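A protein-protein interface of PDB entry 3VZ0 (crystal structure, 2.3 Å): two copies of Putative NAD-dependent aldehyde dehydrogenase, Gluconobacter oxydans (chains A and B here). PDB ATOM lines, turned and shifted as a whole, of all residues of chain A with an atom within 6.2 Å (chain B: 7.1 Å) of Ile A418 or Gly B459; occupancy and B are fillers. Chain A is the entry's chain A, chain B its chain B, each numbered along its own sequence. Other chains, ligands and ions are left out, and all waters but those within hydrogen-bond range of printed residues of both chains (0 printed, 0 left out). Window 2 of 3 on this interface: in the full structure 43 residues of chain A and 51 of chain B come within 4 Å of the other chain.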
ATOM      1  N   GLY A 394      -6.662 -19.757  -5.915  1.00  0.00           N
ATOM      2  CA  GLY A 394      -7.376 -20.120  -4.700  1.00  0.00           C
ATOM      3  C   GLY A 394      -7.479 -21.621  -4.644  1.00  0.00           C
ATOM      4  O   GLY A 394      -7.435 -22.280  -5.676  1.00  0.00           O
ATOM      5  N   ALA A 395      -7.580 -22.165  -3.437  1.00  0.00           N
ATOM      6  CA  ALA A 395      -7.787 -23.594  -3.249  1.00  0.00           C
ATOM      7  C   ALA A 395      -8.855 -23.851  -2.179  1.00  0.00           C
ATOM      8  O   ALA A 395      -8.958 -23.097  -1.198  1.00  0.00           O
ATOM      9  CB  ALA A 395      -6.478 -24.285  -2.904  1.00  0.00           C
ATOM     10  N   VAL A 396      -9.674 -24.884  -2.391  1.00  0.00           N
ATOM     11  CA  VAL A 396     -10.640 -25.304  -1.375  1.00  0.00           C
ATOM     12  C   VAL A 396     -10.494 -26.787  -1.086  1.00  0.00           C
ATOM     13  O   VAL A 396     -10.463 -27.579  -2.008  1.00  0.00           O
ATOM     14  CB  VAL A 396     -12.117 -24.994  -1.780  1.00  0.00           C
ATOM     15  CG1 VAL A 396     -13.081 -25.377  -0.637  1.00  0.00           C
ATOM     16  CG2 VAL A 396     -12.289 -23.520  -2.134  1.00  0.00           C
ATOM     17  N   PHE A 397     -10.393 -27.134   0.203  1.00  0.00           N
ATOM     18  CA  PHE A 397     -10.334 -28.528   0.675  1.00  0.00           C
ATOM     19  C   PHE A 397     -11.554 -28.954   1.516  1.00  0.00           C
ATOM     20  O   PHE A 397     -11.847 -28.374   2.563  1.00  0.00           O
ATOM     21  CB  PHE A 397      -9.017 -28.820   1.414  1.00  0.00           C
ATOM     22  CG  PHE A 397      -7.816 -28.888   0.499  1.00  0.00           C
ATOM     23  CD1 PHE A 397      -7.299 -27.736  -0.083  1.00  0.00           C
ATOM     24  CD2 PHE A 397      -7.222 -30.104   0.201  1.00  0.00           C
ATOM     25  CE1 PHE A 397      -6.213 -27.809  -0.951  1.00  0.00           C
ATOM     26  CE2 PHE A 397      -6.128 -30.170  -0.660  1.00  0.00           C
ATOM     27  CZ  PHE A 397      -5.632 -29.018  -1.230  1.00  0.00           C
ATOM     28  N   SER A 398     -12.244 -29.986   1.024  1.00  0.00           N
ATOM     29  CA  SER A 398     -13.451 -30.556   1.628  1.00  0.00           C
ATOM     30  C   SER A 398     -13.685 -31.913   0.977  1.00  0.00           C
ATOM     31  O   SER A 398     -13.583 -32.031  -0.246  1.00  0.00           O
ATOM     32  CB  SER A 398     -14.656 -29.659   1.335  1.00  0.00           C
ATOM     33  OG  SER A 398     -15.869 -30.265   1.755  1.00  0.00           O
ATOM     34  N   ASP A 400     -16.515 -33.125   0.768  1.00  0.00           N
ATOM     35  CA  ASP A 400     -17.798 -32.909   0.124  1.00  0.00           C
ATOM     36  C   ASP A 400     -17.571 -32.023  -1.117  1.00  0.00           C
ATOM     37  O   ASP A 400     -17.303 -30.827  -0.994  1.00  0.00           O
ATOM     38  CB  ASP A 400     -18.744 -32.266   1.131  1.00  0.00           C
ATOM     39  CG  ASP A 400     -20.109 -31.978   0.565  1.00  0.00           C
ATOM     40  OD1 ASP A 400     -20.342 -32.193  -0.638  1.00  0.00           O
ATOM     41  OD2 ASP A 400     -20.973 -31.530   1.349  1.00  0.00           O
ATOM     42  N   ILE A 401     -17.662 -32.627  -2.303  1.00  0.00           N
ATOM     43  CA  ILE A 401     -17.255 -31.964  -3.538  1.00  0.00           C
ATOM     44  C   ILE A 401     -18.172 -30.813  -3.882  1.00  0.00           C
ATOM     45  O   ILE A 401     -17.705 -29.770  -4.351  1.00  0.00           O
ATOM     46  CB  ILE A 401     -17.125 -32.946  -4.737  1.00  0.00           C
ATOM     47  CG1 ILE A 401     -16.107 -34.043  -4.423  1.00  0.00           C
ATOM     48  CG2 ILE A 401     -16.686 -32.207  -6.011  1.00  0.00           C
ATOM     49  CD1 ILE A 401     -14.769 -33.534  -3.896  1.00  0.00           C
ATOM     50  N   ALA A 404     -17.387 -27.841  -1.681  1.00  0.00           N
ATOM     51  CA  ALA A 404     -16.177 -27.215  -2.199  1.00  0.00           C
ATOM     52  C   ALA A 404     -16.491 -26.426  -3.474  1.00  0.00           C
ATOM     53  O   ALA A 404     -15.976 -25.339  -3.674  1.00  0.00           O
ATOM     54  CB  ALA A 404     -15.111 -28.281  -2.460  1.00  0.00           C
ATOM     55  N   GLU A 405     -17.354 -26.979  -4.317  1.00  0.00           N
ATOM     56  CA  GLU A 405     -17.864 -26.274  -5.491  1.00  0.00           C
ATOM     57  C   GLU A 405     -18.566 -24.956  -5.148  1.00  0.00           C
ATOM     58  O   GLU A 405     -18.346 -23.951  -5.810  1.00  0.00           O
ATOM     59  CB  GLU A 405     -18.829 -27.167  -6.277  1.00  0.00           C
ATOM     60  CG  GLU A 405     -19.493 -26.447  -7.449  1.00  0.00           C
ATOM     61  CD  GLU A 405     -18.484 -26.091  -8.529  1.00  0.00           C
ATOM     62  OE1 GLU A 405     -17.869 -27.045  -9.059  1.00  0.00           O
ATOM     63  OE2 GLU A 405     -18.296 -24.874  -8.832  1.00  0.00           O
ATOM     64  N   ALA A 408     -16.117 -22.473  -4.017  1.00  0.00           N
ATOM     65  CA  ALA A 408     -15.364 -22.035  -5.189  1.00  0.00           C
ATOM     66  C   ALA A 408     -16.111 -20.925  -5.958  1.00  0.00           C
ATOM     67  O   ALA A 408     -15.504 -19.952  -6.419  1.00  0.00           O
ATOM     68  CB  ALA A 408     -15.047 -23.241  -6.106  1.00  0.00           C
ATOM     69  N   VAL A 416      -9.929 -21.423  -9.001  1.00  0.00           N
ATOM     70  CA  VAL A 416     -10.044 -22.145  -7.728  1.00  0.00           C
ATOM     71  C   VAL A 416      -9.792 -23.627  -7.945  1.00  0.00           C
ATOM     72  O   VAL A 416     -10.434 -24.263  -8.779  1.00  0.00           O
ATOM     73  CB  VAL A 416     -11.420 -21.940  -7.008  1.00  0.00           C
ATOM     74  CG1 VAL A 416     -11.415 -22.648  -5.659  1.00  0.00           C
ATOM     75  CG2 VAL A 416     -11.749 -20.445  -6.792  1.00  0.00           C
ATOM     76  N   PHE A 417      -8.832 -24.169  -7.202  1.00  0.00           N
ATOM     77  CA  PHE A 417      -8.530 -25.592  -7.274  1.00  0.00           C
ATOM     78  C   PHE A 417      -9.160 -26.343  -6.094  1.00  0.00           C
ATOM     79  O   PHE A 417      -9.100 -25.891  -4.940  1.00  0.00           O
ATOM     80  CB  PHE A 417      -7.014 -25.822  -7.368  1.00  0.00           C
ATOM     81  CG  PHE A 417      -6.426 -25.465  -8.720  1.00  0.00           C
ATOM     82  CD1 PHE A 417      -6.471 -24.152  -9.199  1.00  0.00           C
ATOM     83  CD2 PHE A 417      -5.820 -26.443  -9.504  1.00  0.00           C
ATOM     84  CE1 PHE A 417      -5.926 -23.820 -10.445  1.00  0.00           C
ATOM     85  CE2 PHE A 417      -5.281 -26.131 -10.756  1.00  0.00           C
ATOM     86  CZ  PHE A 417      -5.334 -24.805 -11.224  1.00  0.00           C
ATOM     87  N   ILE A 418      -9.788 -27.467  -6.404  1.00  0.00           N
ATOM     88  CA  ILE A 418     -10.469 -28.250  -5.392  1.00  0.00           C
ATOM     89  C   ILE A 418      -9.699 -29.521  -5.029  1.00  0.00           C
ATOM     90  O   ILE A 418      -9.460 -30.393  -5.854  1.00  0.00           O
ATOM     91  CB  ILE A 418     -11.938 -28.550  -5.770  1.00  0.00           C
ATOM     92  CG1 ILE A 418     -12.732 -27.237  -5.859  1.00  0.00           C
ATOM     93  CG2 ILE A 418     -12.601 -29.558  -4.741  1.00  0.00           C
ATOM     94  CD1 ILE A 418     -14.147 -27.379  -6.470  1.00  0.00           C
ATOM     95  N   ASN A 419      -9.340 -29.593  -3.753  1.00  0.00           N
ATOM     96  CA  ASN A 419      -8.567 -30.678  -3.188  1.00  0.00           C
ATOM     97  C   ASN A 419      -7.171 -30.871  -3.760  1.00  0.00           C
ATOM     98  O   ASN A 419      -6.543 -31.856  -3.507  1.00  0.00           O
ATOM     99  CB  ASN A 419      -9.381 -31.987  -3.164  1.00  0.00           C
ATOM    100  CG  ASN A 419     -10.532 -31.918  -2.207  1.00  0.00           C
ATOM    101  OD1 ASN A 419     -10.438 -31.272  -1.153  1.00  0.00           O
ATOM    102  ND2 ASN A 419     -11.647 -32.570  -2.563  1.00  0.00           N
ATOM    103  N   THR A 420      -6.706 -29.913  -4.543  1.00  0.00           N
ATOM    104  CA  THR A 420      -5.277 -29.732  -4.843  1.00  0.00           C
ATOM    105  C   THR A 420      -4.942 -28.249  -4.650  1.00  0.00           C
ATOM    106  O   THR A 420      -5.849 -27.421  -4.465  1.00  0.00           O
ATOM    107  CB  THR A 420      -4.893 -30.108  -6.310  1.00  0.00           C
ATOM    108  OG1 THR A 420      -5.844 -29.538  -7.216  1.00  0.00           O
ATOM    109  CG2 THR A 420      -4.882 -31.595  -6.502  1.00  0.00           C
ATOM    110  N   THR B 116      -6.501 -35.131 -16.618  1.00  0.00           N
ATOM    111  CA  THR B 116      -6.876 -35.815 -15.373  1.00  0.00           C
ATOM    112  C   THR B 116      -7.889 -34.968 -14.630  1.00  0.00           C
ATOM    113  O   THR B 116      -7.891 -33.750 -14.774  1.00  0.00           O
ATOM    114  CB  THR B 116      -5.670 -35.999 -14.421  1.00  0.00           C
ATOM    115  OG1 THR B 116      -4.963 -34.751 -14.297  1.00  0.00           O
ATOM    116  CG2 THR B 116      -4.723 -37.101 -14.912  1.00  0.00           C
ATOM    117  N   GLY B 117      -8.724 -35.606 -13.813  1.00  0.00           N
ATOM    118  CA  GLY B 117      -9.784 -34.905 -13.078  1.00  0.00           C
ATOM    119  C   GLY B 117     -10.801 -34.188 -13.960  1.00  0.00           C
ATOM    120  O   GLY B 117     -11.185 -34.688 -15.026  1.00  0.00           O
ATOM    121  N   GLN B 118     -11.244 -33.023 -13.495  1.00  0.00           N
ATOM    122  CA  GLN B 118     -12.194 -32.191 -14.217  1.00  0.00           C
ATOM    123  C   GLN B 118     -11.808 -30.733 -14.114  1.00  0.00           C
ATOM    124  O   GLN B 118     -11.213 -30.314 -13.112  1.00  0.00           O
ATOM    125  CB  GLN B 118     -13.589 -32.295 -13.610  1.00  0.00           C
ATOM    126  CG  GLN B 118     -14.162 -33.676 -13.503  1.00  0.00           C
ATOM    127  CD  GLN B 118     -15.359 -33.714 -12.566  1.00  0.00           C
ATOM    128  OE1 GLN B 118     -16.180 -32.779 -12.541  1.00  0.00           O
ATOM    129  NE2 GLN B 118     -15.463 -34.784 -11.788  1.00  0.00           N
ATOM    130  N   ALA B 119     -12.207 -29.964 -15.127  1.00  0.00           N
ATOM    131  CA  ALA B 119     -12.106 -28.511 -15.102  1.00  0.00           C
ATOM    132  C   ALA B 119     -13.230 -27.832 -15.904  1.00  0.00           C
ATOM    133  O   ALA B 119     -13.681 -28.335 -16.926  1.00  0.00           O
ATOM    134  CB  ALA B 119     -10.740 -28.064 -15.588  1.00  0.00           C
ATOM    135  N   LYS B 120     -13.700 -26.700 -15.413  1.00  0.00           N
ATOM    136  CA  LYS B 120     -14.679 -25.902 -16.138  1.00  0.00           C
ATOM    137  C   LYS B 120     -14.358 -24.450 -15.949  1.00  0.00           C
ATOM    138  O   LYS B 120     -13.640 -24.100 -15.029  1.00  0.00           O
ATOM    139  CB  LYS B 120     -16.108 -26.165 -15.653  1.00  0.00           C
ATOM    140  CG  LYS B 120     -16.387 -25.834 -14.180  1.00  0.00           C
ATOM    141  CD  LYS B 120     -17.856 -26.125 -13.850  1.00  0.00           C
ATOM    142  CE  LYS B 120     -18.198 -25.915 -12.377  1.00  0.00           C
ATOM    143  NZ  LYS B 120     -18.213 -27.202 -11.616  1.00  0.00           N
ATOM    144  N   VAL B 456     -12.524 -23.482 -12.464  1.00  0.00           N
ATOM    145  CA  VAL B 456     -12.790 -24.337 -11.316  1.00  0.00           C
ATOM    146  C   VAL B 456     -12.292 -25.709 -11.679  1.00  0.00           C
ATOM    147  O   VAL B 456     -12.815 -26.351 -12.596  1.00  0.00           O
ATOM    148  CB  VAL B 456     -14.294 -24.392 -10.904  1.00  0.00           C
ATOM    149  CG1 VAL B 456     -14.487 -25.308  -9.714  1.00  0.00           C
ATOM    150  CG2 VAL B 456     -14.829 -23.001 -10.601  1.00  0.00           C
ATOM    151  N   ARG B 457     -11.286 -26.156 -10.938  1.00  0.00           N
ATOM    152  CA  ARG B 457     -10.544 -27.329 -11.287  1.00  0.00           C
ATOM    153  C   ARG B 457     -10.484 -28.318 -10.116  1.00  0.00           C
ATOM    154  O   ARG B 457     -10.013 -27.987  -9.028  1.00  0.00           O
ATOM    155  CB  ARG B 457      -9.172 -26.874 -11.830  1.00  0.00           C
ATOM    156  CG  ARG B 457      -7.945 -27.779 -11.681  1.00  0.00           C
ATOM    157  CD  ARG B 457      -8.190 -29.205 -11.916  1.00  0.00           C
ATOM    158  NE  ARG B 457      -6.981 -29.933 -12.280  1.00  0.00           N
ATOM    159  CZ  ARG B 457      -6.971 -30.856 -13.229  1.00  0.00           C
ATOM    160  NH1 ARG B 457      -8.098 -31.139 -13.883  1.00  0.00           N
ATOM    161  NH2 ARG B 457      -5.852 -31.485 -13.527  1.00  0.00           N
ATOM    162  N   ILE B 458     -11.010 -29.524 -10.352  1.00  0.00           N
ATOM    163  CA  ILE B 458     -10.925 -30.652  -9.409  1.00  0.00           C
ATOM    164  C   ILE B 458      -9.905 -31.649  -9.942  1.00  0.00           C
ATOM    165  O   ILE B 458     -10.153 -32.344 -10.927  1.00  0.00           O
ATOM    166  CB  ILE B 458     -12.296 -31.373  -9.222  1.00  0.00           C
ATOM    167  CG1 ILE B 458     -13.439 -30.347  -9.105  1.00  0.00           C
ATOM    168  CG2 ILE B 458     -12.242 -32.339  -8.027  1.00  0.00           C
ATOM    169  CD1 ILE B 458     -14.822 -30.916  -9.337  1.00  0.00           C
ATOM    170  N   GLY B 459      -8.751 -31.717  -9.289  1.00  0.00           N
ATOM    171  CA  GLY B 459      -7.656 -32.570  -9.751  1.00  0.00           C
ATOM    172  C   GLY B 459      -7.905 -34.046  -9.473  1.00  0.00           C
ATOM    173  O   GLY B 459      -8.427 -34.412  -8.409  1.00  0.00           O
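The side-chain carboxylate of Glu A405 is in salt-bridge range of the side-chain amino group of Lys B120, 2.6 Å away. The backbone carbonyl oxygen of Val A416 is in hydrogen-bond range of the backbone NH of Arg B457, at 3.0 Å. N of Ile A418 sits at hydrogen-bond distance from O of Arg B457 (2.7 Å).
The backbone NH of Phe A417 sits at hydrogen-bond distance from the backbone carbonyl oxygen of Gly A394 (2.8 Å). The backbone NH (N) of Val A396 is in hydrogen-bond range of the backbone carbonyl oxygen (O) of Phe A417. The backbone carbonyl oxygen (O) of Thr B116 is in hydrogen-bond range of the guanidinium group (NH1) of Arg B457, at 2.8 Å. The backbone carbonyl oxygen (O) of Gln B118 lies within hydrogen-bond range of the guanidinium group (NH1) of Arg B457. The backbone carbonyl oxygen (O) of Ile B458 sits at hydrogen-bond distance from the backbone NH (N) of Gln B118 (2.9 Å). The backbone carbonyl oxygen (O) of Lys B120 sits at hydrogen-bond distance from the backbone NH (N) of Val B456 (2.9 Å).
Val B456 touches Glu A405 (CG1 to OE1, 3.9 Å). Val B456 touches Val A416. Arg B457 touches Phe A417. CD1 of Ile A418 touches CG1 of Val B456, at 3.9 Å. Ile B458 touches Ile A418 (CA to O, 3.9 Å). Ile A418 touches Gly B459 (O to N, 3.7 Å).
Ala A408 touches none of the printed residues of chain B. Printed residues of chain B within 4 Å of Val A416: Val B456 (3.5 Å) and Arg B457 (3.0 Å). Of chain B, only Val B456 (3.9 Å), Arg B457 (2.7 Å), Ile B458 (3.9 Å) and Gly B459 (3.7 Å) come within 4 Å of Ile A418. Ala B119 touches none of the printed residues of chain A. Printed residues of chain A within 4 Å of Ile B458: Ile A418. The nearest residue of chain A that does not touch Gly B459 is Thr A420 (4.2 Å). The nearest printed residue of chain A that does not touch Lys B120 is Ile A418 (6.6 Å).
Hydrophobic or aromatic side chains of chain B that line the printed part of chain A: Val B456. Among the printed residues, 9 pairs touch across the chains. Among the printed residues, Asp or Glu carboxylates within 4 Å of a Lys or Arg side-chain nitrogen of the other chain: Glu A405 with Lys B120.
No position is printed for both chains.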
